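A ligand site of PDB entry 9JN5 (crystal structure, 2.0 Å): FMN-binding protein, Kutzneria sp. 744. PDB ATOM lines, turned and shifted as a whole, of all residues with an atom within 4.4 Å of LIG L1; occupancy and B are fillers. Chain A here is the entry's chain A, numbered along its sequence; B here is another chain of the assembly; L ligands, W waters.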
ATOM      1  N   LEU A  29       0.705  -9.773  -4.995  1.00  0.00           N
ATOM      2  CA  LEU A  29       1.095  -9.296  -6.344  1.00  0.00           C
ATOM      3  C   LEU A  29      -0.165  -9.283  -7.216  1.00  0.00           C
ATOM      4  O   LEU A  29      -0.455 -10.285  -7.901  1.00  0.00           O
ATOM      5  CB  LEU A  29       2.229 -10.116  -6.925  1.00  0.00           C
ATOM      6  CG  LEU A  29       2.885  -9.457  -8.131  1.00  0.00           C
ATOM      7  CD1 LEU A  29       3.658  -8.188  -7.735  1.00  0.00           C
ATOM      8  CD2 LEU A  29       3.777 -10.431  -8.872  1.00  0.00           C
ATOM      9  N   THR A  45      -0.549  -3.492 -14.691  1.00  0.00           N
ATOM     10  CA  THR A  45       0.738  -3.563 -13.980  1.00  0.00           C
ATOM     11  C   THR A  45       0.601  -4.509 -12.794  1.00  0.00           C
ATOM     12  O   THR A  45      -0.372  -4.360 -12.024  1.00  0.00           O
ATOM     13  CB  THR A  45       1.252  -2.194 -13.508  1.00  0.00           C
ATOM     14  OG1 THR A  45       1.196  -1.266 -14.601  1.00  0.00           O
ATOM     15  CG2 THR A  45       2.679  -2.269 -12.987  1.00  0.00           C
ATOM     16  N   HIS A  46       1.546  -5.437 -12.675  1.00  0.00           N
ATOM     17  CA  HIS A  46       1.722  -6.329 -11.498  1.00  0.00           C
ATOM     18  C   HIS A  46       2.317  -5.463 -10.382  1.00  0.00           C
ATOM     19  O   HIS A  46       3.423  -4.955 -10.525  1.00  0.00           O
ATOM     20  CB  HIS A  46       2.561  -7.569 -11.846  1.00  0.00           C
ATOM     21  CG  HIS A  46       1.764  -8.696 -12.454  1.00  0.00           C
ATOM     22  ND1 HIS A  46       1.546  -8.802 -13.806  1.00  0.00           N
ATOM     23  CD2 HIS A  46       1.142  -9.753 -11.897  1.00  0.00           C
ATOM     24  CE1 HIS A  46       0.787  -9.868 -14.067  1.00  0.00           C
ATOM     25  NE2 HIS A  46       0.570 -10.480 -12.909  1.00  0.00           N
ATOM     26  N   PRO A  48       2.590  -4.838  -5.859  1.00  0.00           N
ATOM     27  CA  PRO A  48       2.355  -5.381  -4.539  1.00  0.00           C
ATOM     28  C   PRO A  48       1.360  -4.524  -3.754  1.00  0.00           C
ATOM     29  O   PRO A  48       1.595  -3.341  -3.561  1.00  0.00           O
ATOM     30  CB  PRO A  48       3.714  -5.360  -3.840  1.00  0.00           C
ATOM     31  CG  PRO A  48       4.464  -4.275  -4.535  1.00  0.00           C
ATOM     32  CD  PRO A  48       3.903  -4.182  -5.947  1.00  0.00           C
ATOM     33  N   HIS A  70       2.430   0.133  -4.340  1.00  0.00           N
ATOM     34  CA  HIS A  70       3.332   1.007  -5.131  1.00  0.00           C
ATOM     35  C   HIS A  70       3.609   0.385  -6.477  1.00  0.00           C
ATOM     36  O   HIS A  70       3.348  -0.814  -6.658  1.00  0.00           O
ATOM     37  CB  HIS A  70       4.605   1.348  -4.362  1.00  0.00           C
ATOM     38  CG  HIS A  70       5.555   0.210  -4.216  1.00  0.00           C
ATOM     39  ND1 HIS A  70       5.362  -0.786  -3.277  1.00  0.00           N
ATOM     40  CD2 HIS A  70       6.728  -0.068  -4.854  1.00  0.00           C
ATOM     41  CE1 HIS A  70       6.377  -1.640  -3.348  1.00  0.00           C
ATOM     42  NE2 HIS A  70       7.209  -1.227  -4.309  1.00  0.00           N
ATOM     43  N   MET A  71       4.126   1.217  -7.381  1.00  0.00           N
ATOM     44  CA  MET A  71       4.590   0.838  -8.714  1.00  0.00           C
ATOM     45  C   MET A  71       5.755   1.761  -9.046  1.00  0.00           C
ATOM     46  O   MET A  71       6.088   2.613  -8.203  1.00  0.00           O
ATOM     47  CB  MET A  71       3.472   0.983  -9.759  1.00  0.00           C
ATOM     48  CG  MET A  71       2.987   2.412 -10.007  1.00  0.00           C
ATOM     49  SD  MET A  71       2.011   2.507 -11.503  1.00  0.00           S
ATOM     50  CE  MET A  71       0.484   1.893 -10.799  1.00  0.00           C
ATOM     51  N   ASN A  72       6.303   1.597 -10.248  1.00  0.00           N
ATOM     52  CA  ASN A  72       7.396   2.436 -10.779  1.00  0.00           C
ATOM     53  C   ASN A  72       6.807   3.750 -11.324  1.00  0.00           C
ATOM     54  O   ASN A  72       6.007   3.672 -12.256  1.00  0.00           O
ATOM     55  CB  ASN A  72       8.198   1.742 -11.866  1.00  0.00           C
ATOM     56  CG  ASN A  72       9.465   2.506 -12.142  1.00  0.00           C
ATOM     57  OD1 ASN A  72       9.527   3.710 -11.843  1.00  0.00           O
ATOM     58  ND2 ASN A  72      10.473   1.804 -12.642  1.00  0.00           N
ATOM     59  N   ASN A  75       7.030   3.963 -14.933  1.00  0.00           N
ATOM     60  CA  ASN A  75       5.946   3.189 -15.604  1.00  0.00           C
ATOM     61  C   ASN A  75       4.924   4.157 -16.194  1.00  0.00           C
ATOM     62  O   ASN A  75       4.247   4.857 -15.437  1.00  0.00           O
ATOM     63  CB  ASN A  75       5.296   2.224 -14.620  1.00  0.00           C
ATOM     64  CG  ASN A  75       4.402   1.202 -15.288  1.00  0.00           C
ATOM     65  OD1 ASN A  75       3.801   1.525 -16.309  1.00  0.00           O
ATOM     66  ND2 ASN A  75       4.299   0.009 -14.693  1.00  0.00           N
ATOM     67  N   VAL A 136       6.336   1.383   1.450  1.00  0.00           N
ATOM     68  CA  VAL A 136       7.293   0.263   1.169  1.00  0.00           C
ATOM     69  C   VAL A 136       7.673  -0.462   2.479  1.00  0.00           C
ATOM     70  O   VAL A 136       7.801  -1.682   2.402  1.00  0.00           O
ATOM     71  CB  VAL A 136       8.512   0.640   0.297  1.00  0.00           C
ATOM     72  CG1 VAL A 136       8.060   1.173  -1.046  1.00  0.00           C
ATOM     73  CG2 VAL A 136       9.505   1.586   0.958  1.00  0.00           C
ATOM     74  N   THR A 139       4.767  -2.823   3.378  1.00  0.00           N
ATOM     75  CA  THR A 139       4.923  -3.891   2.340  1.00  0.00           C
ATOM     76  C   THR A 139       6.049  -4.862   2.717  1.00  0.00           C
ATOM     77  O   THR A 139       5.850  -6.081   2.576  1.00  0.00           O
ATOM     78  CB  THR A 139       5.177  -3.284   0.952  1.00  0.00           C
ATOM     79  OG1 THR A 139       4.106  -2.379   0.768  1.00  0.00           O
ATOM     80  CG2 THR A 139       5.178  -4.271  -0.186  1.00  0.00           C
ATOM     81  N   VAL A 140       7.206  -4.378   3.153  1.00  0.00           N
ATOM     82  CA  VAL A 140       8.273  -5.294   3.652  1.00  0.00           C
ATOM     83  C   VAL A 140       7.714  -6.033   4.884  1.00  0.00           C
ATOM     84  O   VAL A 140       7.773  -7.245   4.911  1.00  0.00           O
ATOM     85  CB  VAL A 140       9.613  -4.579   3.913  1.00  0.00           C
ATOM     86  CG1 VAL A 140      10.544  -5.513   4.648  1.00  0.00           C
ATOM     87  CG2 VAL A 140      10.273  -4.087   2.618  1.00  0.00           C
ATOM     88  N   LEU A 143       4.868  -8.684   3.765  1.00  0.00           N
ATOM     89  CA  LEU A 143       5.265  -9.789   2.846  1.00  0.00           C
ATOM     90  C   LEU A 143       6.409 -10.619   3.442  1.00  0.00           C
ATOM     91  O   LEU A 143       6.387 -11.871   3.247  1.00  0.00           O
ATOM     92  CB  LEU A 143       5.641  -9.291   1.452  1.00  0.00           C
ATOM     93  CG  LEU A 143       4.659  -8.394   0.704  1.00  0.00           C
ATOM     94  CD1 LEU A 143       4.878  -8.526  -0.775  1.00  0.00           C
ATOM     95  CD2 LEU A 143       3.204  -8.603   1.096  1.00  0.00           C
ATOM     96  N   PHE A 160      16.516   2.412   1.365  1.00  0.00           N
ATOM     97  CA  PHE A 160      15.097   2.653   0.986  1.00  0.00           C
ATOM     98  C   PHE A 160      14.982   4.149   0.628  1.00  0.00           C
ATOM     99  O   PHE A 160      14.405   4.500  -0.410  1.00  0.00           O
ATOM    100  CB  PHE A 160      14.093   2.254   2.093  1.00  0.00           C
ATOM    101  CG  PHE A 160      13.876   0.782   2.411  1.00  0.00           C
ATOM    102  CD1 PHE A 160      14.638  -0.224   1.841  1.00  0.00           C
ATOM    103  CD2 PHE A 160      12.951   0.419   3.387  1.00  0.00           C
ATOM    104  CE1 PHE A 160      14.454  -1.552   2.181  1.00  0.00           C
ATOM    105  CE2 PHE A 160      12.782  -0.898   3.751  1.00  0.00           C
ATOM    106  CZ  PHE A 160      13.521  -1.894   3.135  1.00  0.00           C
ATOM    107  N   ILE A 163      16.475   5.334  -2.821  1.00  0.00           N
ATOM    108  CA  ILE A 163      15.804   4.897  -4.080  1.00  0.00           C
ATOM    109  C   ILE A 163      14.341   5.349  -4.099  1.00  0.00           C
ATOM    110  O   ILE A 163      13.703   5.231  -5.142  1.00  0.00           O
ATOM    111  CB  ILE A 163      15.939   3.374  -4.287  1.00  0.00           C
ATOM    112  CG1 ILE A 163      15.234   2.567  -3.215  1.00  0.00           C
ATOM    113  CG2 ILE A 163      17.401   2.982  -4.423  1.00  0.00           C
ATOM    114  CD1 ILE A 163      14.901   1.153  -3.645  1.00  0.00           C
ATOM    115  N   LEU A 164      13.853   5.913  -3.003  1.00  0.00           N
ATOM    116  CA  LEU A 164      12.439   6.333  -2.788  1.00  0.00           C
ATOM    117  C   LEU A 164      11.876   7.251  -3.887  1.00  0.00           C
ATOM    118  O   LEU A 164      10.670   7.219  -4.180  1.00  0.00           O
ATOM    119  CB  LEU A 164      12.417   7.066  -1.454  1.00  0.00           C
ATOM    120  CG  LEU A 164      11.054   7.174  -0.771  1.00  0.00           C
ATOM    121  CD1 LEU A 164      10.483   5.783  -0.519  1.00  0.00           C
ATOM    122  CD2 LEU A 164      11.265   7.938   0.510  1.00  0.00           C
ATOM    123  N   GLY A 166      11.802   7.103  -7.030  1.00  0.00           N
ATOM    124  CA  GLY A 166      11.191   6.330  -8.133  1.00  0.00           C
ATOM    125  C   GLY A 166       9.906   5.618  -7.703  1.00  0.00           C
ATOM    126  O   GLY A 166       9.256   5.023  -8.519  1.00  0.00           O
ATOM    127  N   VAL A 167       9.562   5.651  -6.438  1.00  0.00           N
ATOM    128  CA  VAL A 167       8.350   4.966  -5.950  1.00  0.00           C
ATOM    129  C   VAL A 167       7.120   5.824  -6.292  1.00  0.00           C
ATOM    130  O   VAL A 167       7.102   7.013  -5.909  1.00  0.00           O
ATOM    131  CB  VAL A 167       8.446   4.702  -4.437  1.00  0.00           C
ATOM    132  CG1 VAL A 167       7.204   3.992  -3.916  1.00  0.00           C
ATOM    133  CG2 VAL A 167       9.724   3.943  -4.074  1.00  0.00           C
ATOM    134  N   PHE B   7       4.943  -1.819 -19.649  1.00  0.00           N
ATOM    135  CA  PHE B   7       6.254  -1.349 -19.139  1.00  0.00           C
ATOM    136  C   PHE B   7       7.094  -2.550 -18.706  1.00  0.00           C
ATOM    137  O   PHE B   7       6.737  -3.270 -17.740  1.00  0.00           O
ATOM    138  CB  PHE B   7       6.042  -0.378 -17.982  1.00  0.00           C
ATOM    139  CG  PHE B   7       7.328   0.229 -17.481  1.00  0.00           C
ATOM    140  CD1 PHE B   7       8.144   0.939 -18.345  1.00  0.00           C
ATOM    141  CD2 PHE B   7       7.727   0.073 -16.165  1.00  0.00           C
ATOM    142  CE1 PHE B   7       9.341   1.464 -17.902  1.00  0.00           C
ATOM    143  CE2 PHE B   7       8.909   0.632 -15.725  1.00  0.00           C
ATOM    144  CZ  PHE B   7       9.718   1.319 -16.587  1.00  0.00           C
ATOM    145  N   TYR B  97       8.037 -14.625  -4.078  1.00  0.00           N
ATOM    146  CA  TYR B  97       8.638 -13.623  -3.140  1.00  0.00           C
ATOM    147  C   TYR B  97      10.158 -13.824  -3.046  1.00  0.00           C
ATOM    148  O   TYR B  97      10.668 -14.986  -2.977  1.00  0.00           O
ATOM    149  CB  TYR B  97       8.037 -13.730  -1.752  1.00  0.00           C
ATOM    150  CG  TYR B  97       8.586 -12.675  -0.833  1.00  0.00           C
ATOM    151  CD1 TYR B  97       8.212 -11.358  -1.006  1.00  0.00           C
ATOM    152  CD2 TYR B  97       9.464 -12.969   0.190  1.00  0.00           C
ATOM    153  CE1 TYR B  97       8.725 -10.345  -0.208  1.00  0.00           C
ATOM    154  CE2 TYR B  97       9.975 -11.969   1.016  1.00  0.00           C
ATOM    155  CZ  TYR B  97       9.596 -10.654   0.821  1.00  0.00           C
ATOM    156  OH  TYR B  97       9.988  -9.626   1.637  1.00  0.00           O
ATOM    157  N   ALA B 109      16.739  -4.535  -0.788  1.00  0.00           N
ATOM    158  CA  ALA B 109      15.262  -4.509  -0.645  1.00  0.00           C
ATOM    159  C   ALA B 109      14.694  -5.797  -1.223  1.00  0.00           C
ATOM    160  O   ALA B 109      15.275  -6.396  -2.123  1.00  0.00           O
ATOM    161  CB  ALA B 109      14.694  -3.294  -1.310  1.00  0.00           C
ATOM    162  N   PRO B 110      13.507  -6.242  -0.756  1.00  0.00           N
ATOM    163  CA  PRO B 110      12.948  -7.496  -1.241  1.00  0.00           C
ATOM    164  C   PRO B 110      12.273  -7.215  -2.578  1.00  0.00           C
ATOM    165  O   PRO B 110      12.063  -6.060  -2.907  1.00  0.00           O
ATOM    166  CB  PRO B 110      11.912  -7.868  -0.168  1.00  0.00           C
ATOM    167  CG  PRO B 110      12.147  -6.889   0.955  1.00  0.00           C
ATOM    168  CD  PRO B 110      12.659  -5.653   0.273  1.00  0.00           C
ATOM    169  N   THR B 111      11.933  -8.258  -3.314  1.00  0.00           N
ATOM    170  CA  THR B 111      11.159  -8.115  -4.562  1.00  0.00           C
ATOM    171  C   THR B 111      10.304  -9.350  -4.691  1.00  0.00           C
ATOM    172  O   THR B 111      10.254 -10.161  -3.730  1.00  0.00           O
ATOM    173  CB  THR B 111      12.082  -7.879  -5.766  1.00  0.00           C
ATOM    174  OG1 THR B 111      11.262  -7.367  -6.808  1.00  0.00           O
ATOM    175  CG2 THR B 111      12.800  -9.139  -6.236  1.00  0.00           C
ATOM    176  N   TRP B 112       9.669  -9.461  -5.845  1.00  0.00           N
ATOM    177  CA  TRP B 112       8.813 -10.598  -6.236  1.00  0.00           C
ATOM    178  C   TRP B 112       9.227 -10.965  -7.640  1.00  0.00           C
ATOM    179  O   TRP B 112       9.004 -10.121  -8.519  1.00  0.00           O
ATOM    180  CB  TRP B 112       7.316 -10.239  -6.173  1.00  0.00           C
ATOM    181  CG  TRP B 112       6.473 -11.460  -5.946  1.00  0.00           C
ATOM    182  CD1 TRP B 112       6.284 -12.487  -6.821  1.00  0.00           C
ATOM    183  CD2 TRP B 112       5.719 -11.797  -4.769  1.00  0.00           C
ATOM    184  NE1 TRP B 112       5.462 -13.434  -6.280  1.00  0.00           N
ATOM    185  CE2 TRP B 112       5.106 -13.051  -5.010  1.00  0.00           C
ATOM    186  CE3 TRP B 112       5.474 -11.166  -3.541  1.00  0.00           C
ATOM    187  CZ2 TRP B 112       4.308 -13.681  -4.080  1.00  0.00           C
ATOM    188  CZ3 TRP B 112       4.700 -11.802  -2.599  1.00  0.00           C
ATOM    189  CH2 TRP B 112       4.121 -13.044  -2.867  1.00  0.00           C
HETATM  190  C1  LIG L   1       8.809  -0.850  -8.183  1.00  0.00           C
HETATM  191  C2  LIG L   1       7.563  -4.836  -5.905  1.00  0.00           C
HETATM  192  C3  LIG L   1       9.491  -3.206  -1.623  1.00  0.00           C
HETATM  193  C4  LIG L   1      11.228   0.523  -4.150  1.00  0.00           C
HETATM  194  C5  LIG L   1       8.256  -2.055  -7.907  1.00  0.00           C
HETATM  195  C6  LIG L   1       7.582  -2.880  -8.868  1.00  0.00           C
HETATM  196  C7  LIG L   1       7.301  -4.027  -8.222  1.00  0.00           C
HETATM  197  C8  LIG L   1       7.742  -3.900  -6.879  1.00  0.00           C
HETATM  198  C9  LIG L   1       6.585  -5.236  -8.824  1.00  0.00           C
HETATM  199  C10 LIG L   1       7.353  -2.652 -10.347  1.00  0.00           C
HETATM  200  C11 LIG L   1       5.967  -2.023 -10.613  1.00  0.00           C
HETATM  201  C12 LIG L   1       5.821  -1.610 -12.020  1.00  0.00           C
HETATM  202  O1  LIG L   1       5.460  -0.443 -12.323  1.00  0.00           O
HETATM  203  O2  LIG L   1       6.179  -2.399 -12.931  1.00  0.00           O
HETATM  204  C13 LIG L   1       8.011  -4.704  -4.573  1.00  0.00           C
HETATM  205  C14 LIG L   1       7.763  -5.701  -3.606  1.00  0.00           C
HETATM  206  C15 LIG L   1       8.270  -5.279  -2.431  1.00  0.00           C
HETATM  207  C16 LIG L   1       8.858  -3.952  -2.638  1.00  0.00           C
HETATM  208  C17 LIG L   1       7.053  -7.027  -3.853  1.00  0.00           C
HETATM  209  C18 LIG L   1       8.219  -6.130  -1.238  1.00  0.00           C
HETATM  210  C19 LIG L   1       8.613  -5.835  -0.020  1.00  0.00           C
HETATM  211  C20 LIG L   1      10.120  -2.022  -1.976  1.00  0.00           C
HETATM  212  C21 LIG L   1      10.927  -1.294  -1.144  1.00  0.00           C
HETATM  213  C22 LIG L   1      11.435  -0.206  -1.814  1.00  0.00           C
HETATM  214  C23 LIG L   1      10.929  -0.344  -3.131  1.00  0.00           C
HETATM  215  C24 LIG L   1      11.196  -1.586   0.305  1.00  0.00           C
HETATM  216  C25 LIG L   1      12.250   0.848  -1.119  1.00  0.00           C
HETATM  217  C26 LIG L   1      12.358   2.119  -1.498  1.00  0.00           C
HETATM  218  C27 LIG L   1      10.720   0.408  -5.423  1.00  0.00           C
HETATM  219  C28 LIG L   1      11.119   1.351  -6.469  1.00  0.00           C
HETATM  220  C29 LIG L   1      10.474   0.980  -7.558  1.00  0.00           C
HETATM  221  C30 LIG L   1       9.615  -0.159  -7.198  1.00  0.00           C
HETATM  222  C31 LIG L   1      12.060   2.494  -6.407  1.00  0.00           C
HETATM  223  C32 LIG L   1      10.572   1.649  -8.883  1.00  0.00           C
HETATM  224  C33 LIG L   1      11.033   0.520  -9.799  1.00  0.00           C
HETATM  225  C34 LIG L   1      12.514   0.402  -9.837  1.00  0.00           C
HETATM  226  O3  LIG L   1      12.941  -0.646 -10.352  1.00  0.00           O
HETATM  227  O4  LIG L   1      13.268   1.305  -9.364  1.00  0.00           O
HETATM  228  N1  LIG L   1       8.330  -2.667  -6.663  1.00  0.00           N
HETATM  229  N2  LIG L   1       8.633  -3.666  -3.955  1.00  0.00           N
HETATM  230  N3  LIG L   1      10.124  -1.455  -3.218  1.00  0.00           N
HETATM  231  N4  LIG L   1       9.802  -0.448  -5.871  1.00  0.00           N
HETATM  232 FE1  LIG L   1       9.129  -1.962  -4.986  1.00  0.00          FE
HETATM  233  C1  LG2 L   2      16.117  -2.467  -6.576  1.00  0.00           C
HETATM  234  N1  LG2 L   2      14.175  -2.851  -8.071  1.00  0.00           N
HETATM  235  O1  LG2 L   2      16.546  -1.384  -6.098  1.00  0.00           O
HETATM  236  C2  LG2 L   2      14.589  -2.564  -6.692  1.00  0.00           C
HETATM  237  C3  LG2 L   2      14.113  -3.619  -5.709  1.00  0.00           C
HETATM  238  C4  LG2 L   2      11.981  -3.348  -4.513  1.00  0.00           C
HETATM  239  N2  LG2 L   2      11.287  -3.130  -5.784  1.00  0.00           N
HETATM  240  C5  LG2 L   2      13.433  -2.885  -4.571  1.00  0.00           C
HETATM  241  O2  LG2 L   2      11.920  -2.084  -6.679  1.00  0.00           O
HETATM  242  O3  LG2 L   2      16.800  -3.459  -6.957  1.00  0.00           O
HETATM  243  O   HOH W   1      10.234  -1.174 -12.490  1.00  0.00           O
HETATM  244  O   HOH W   2       8.834  -2.735 -13.955  1.00  0.00           O
HETATM  245  O   HOH W   3      13.319   3.882  -9.762  1.00  0.00           O
HETATM  246  O   HOH W   4       5.407  -4.893 -12.446  1.00  0.00           O
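Merely in contact with LIG L1: Thr 45 (3.4 Å), His 46 (3.6 Å), Pro 48 (3.4 Å), Met 71 (3.5 Å), Val 136 (3.4 Å), Thr 139 (3.7 Å), Val 140 (3.5 Å), Phe 160 (3.3 Å), Ile 163 (3.4 Å), Gly 166 (3.6 Å), Val 167 (3.6 Å), Pro 110 of chain B (3.8 Å) and Trp 112 of chain B (3.97 Å). Within 4 Å of LIG L1: Thr 45, His 46, Pro 48, His 70, Met 71, Asn 72, Asn 75, Val 136, Thr 139, Val 140, Phe 160, Ile 163, Gly 166, Val 167, Pro 110 of chain B and Trp 112 of chain B. The nearest printed residue that does not touch LIG L1 is Leu 143 (4.1 Å).
FE1 of LIG L1 is bound by NE2 of His 70, at 2.2 Å. The side-chain amide nitrogen (ND2) of Asn 75 sits at hydrogen-bond distance from an oxygen (O1) of LIG L1, 2.7 Å away. The backbone NH of Asn 72 is in hydrogen-bond range of an oxygen (O1) of LIG L1, 3.0 Å away.
Water W4 lies within hydrogen-bond range of an oxygen (O2) of LIG L1 (2.7 Å) and the backbone carbonyl oxygen (O) of His 46 (2.8 Å). Water W1 bridges ND2 of Asn 72 (3.0 Å) and O3 of LIG L1 (3.5 Å).
ND2 of Asn 75 sits close to OG1 of Thr 45.
N2 of LG2 L2 binds FE1 of LIG L1 (2.6 Å).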
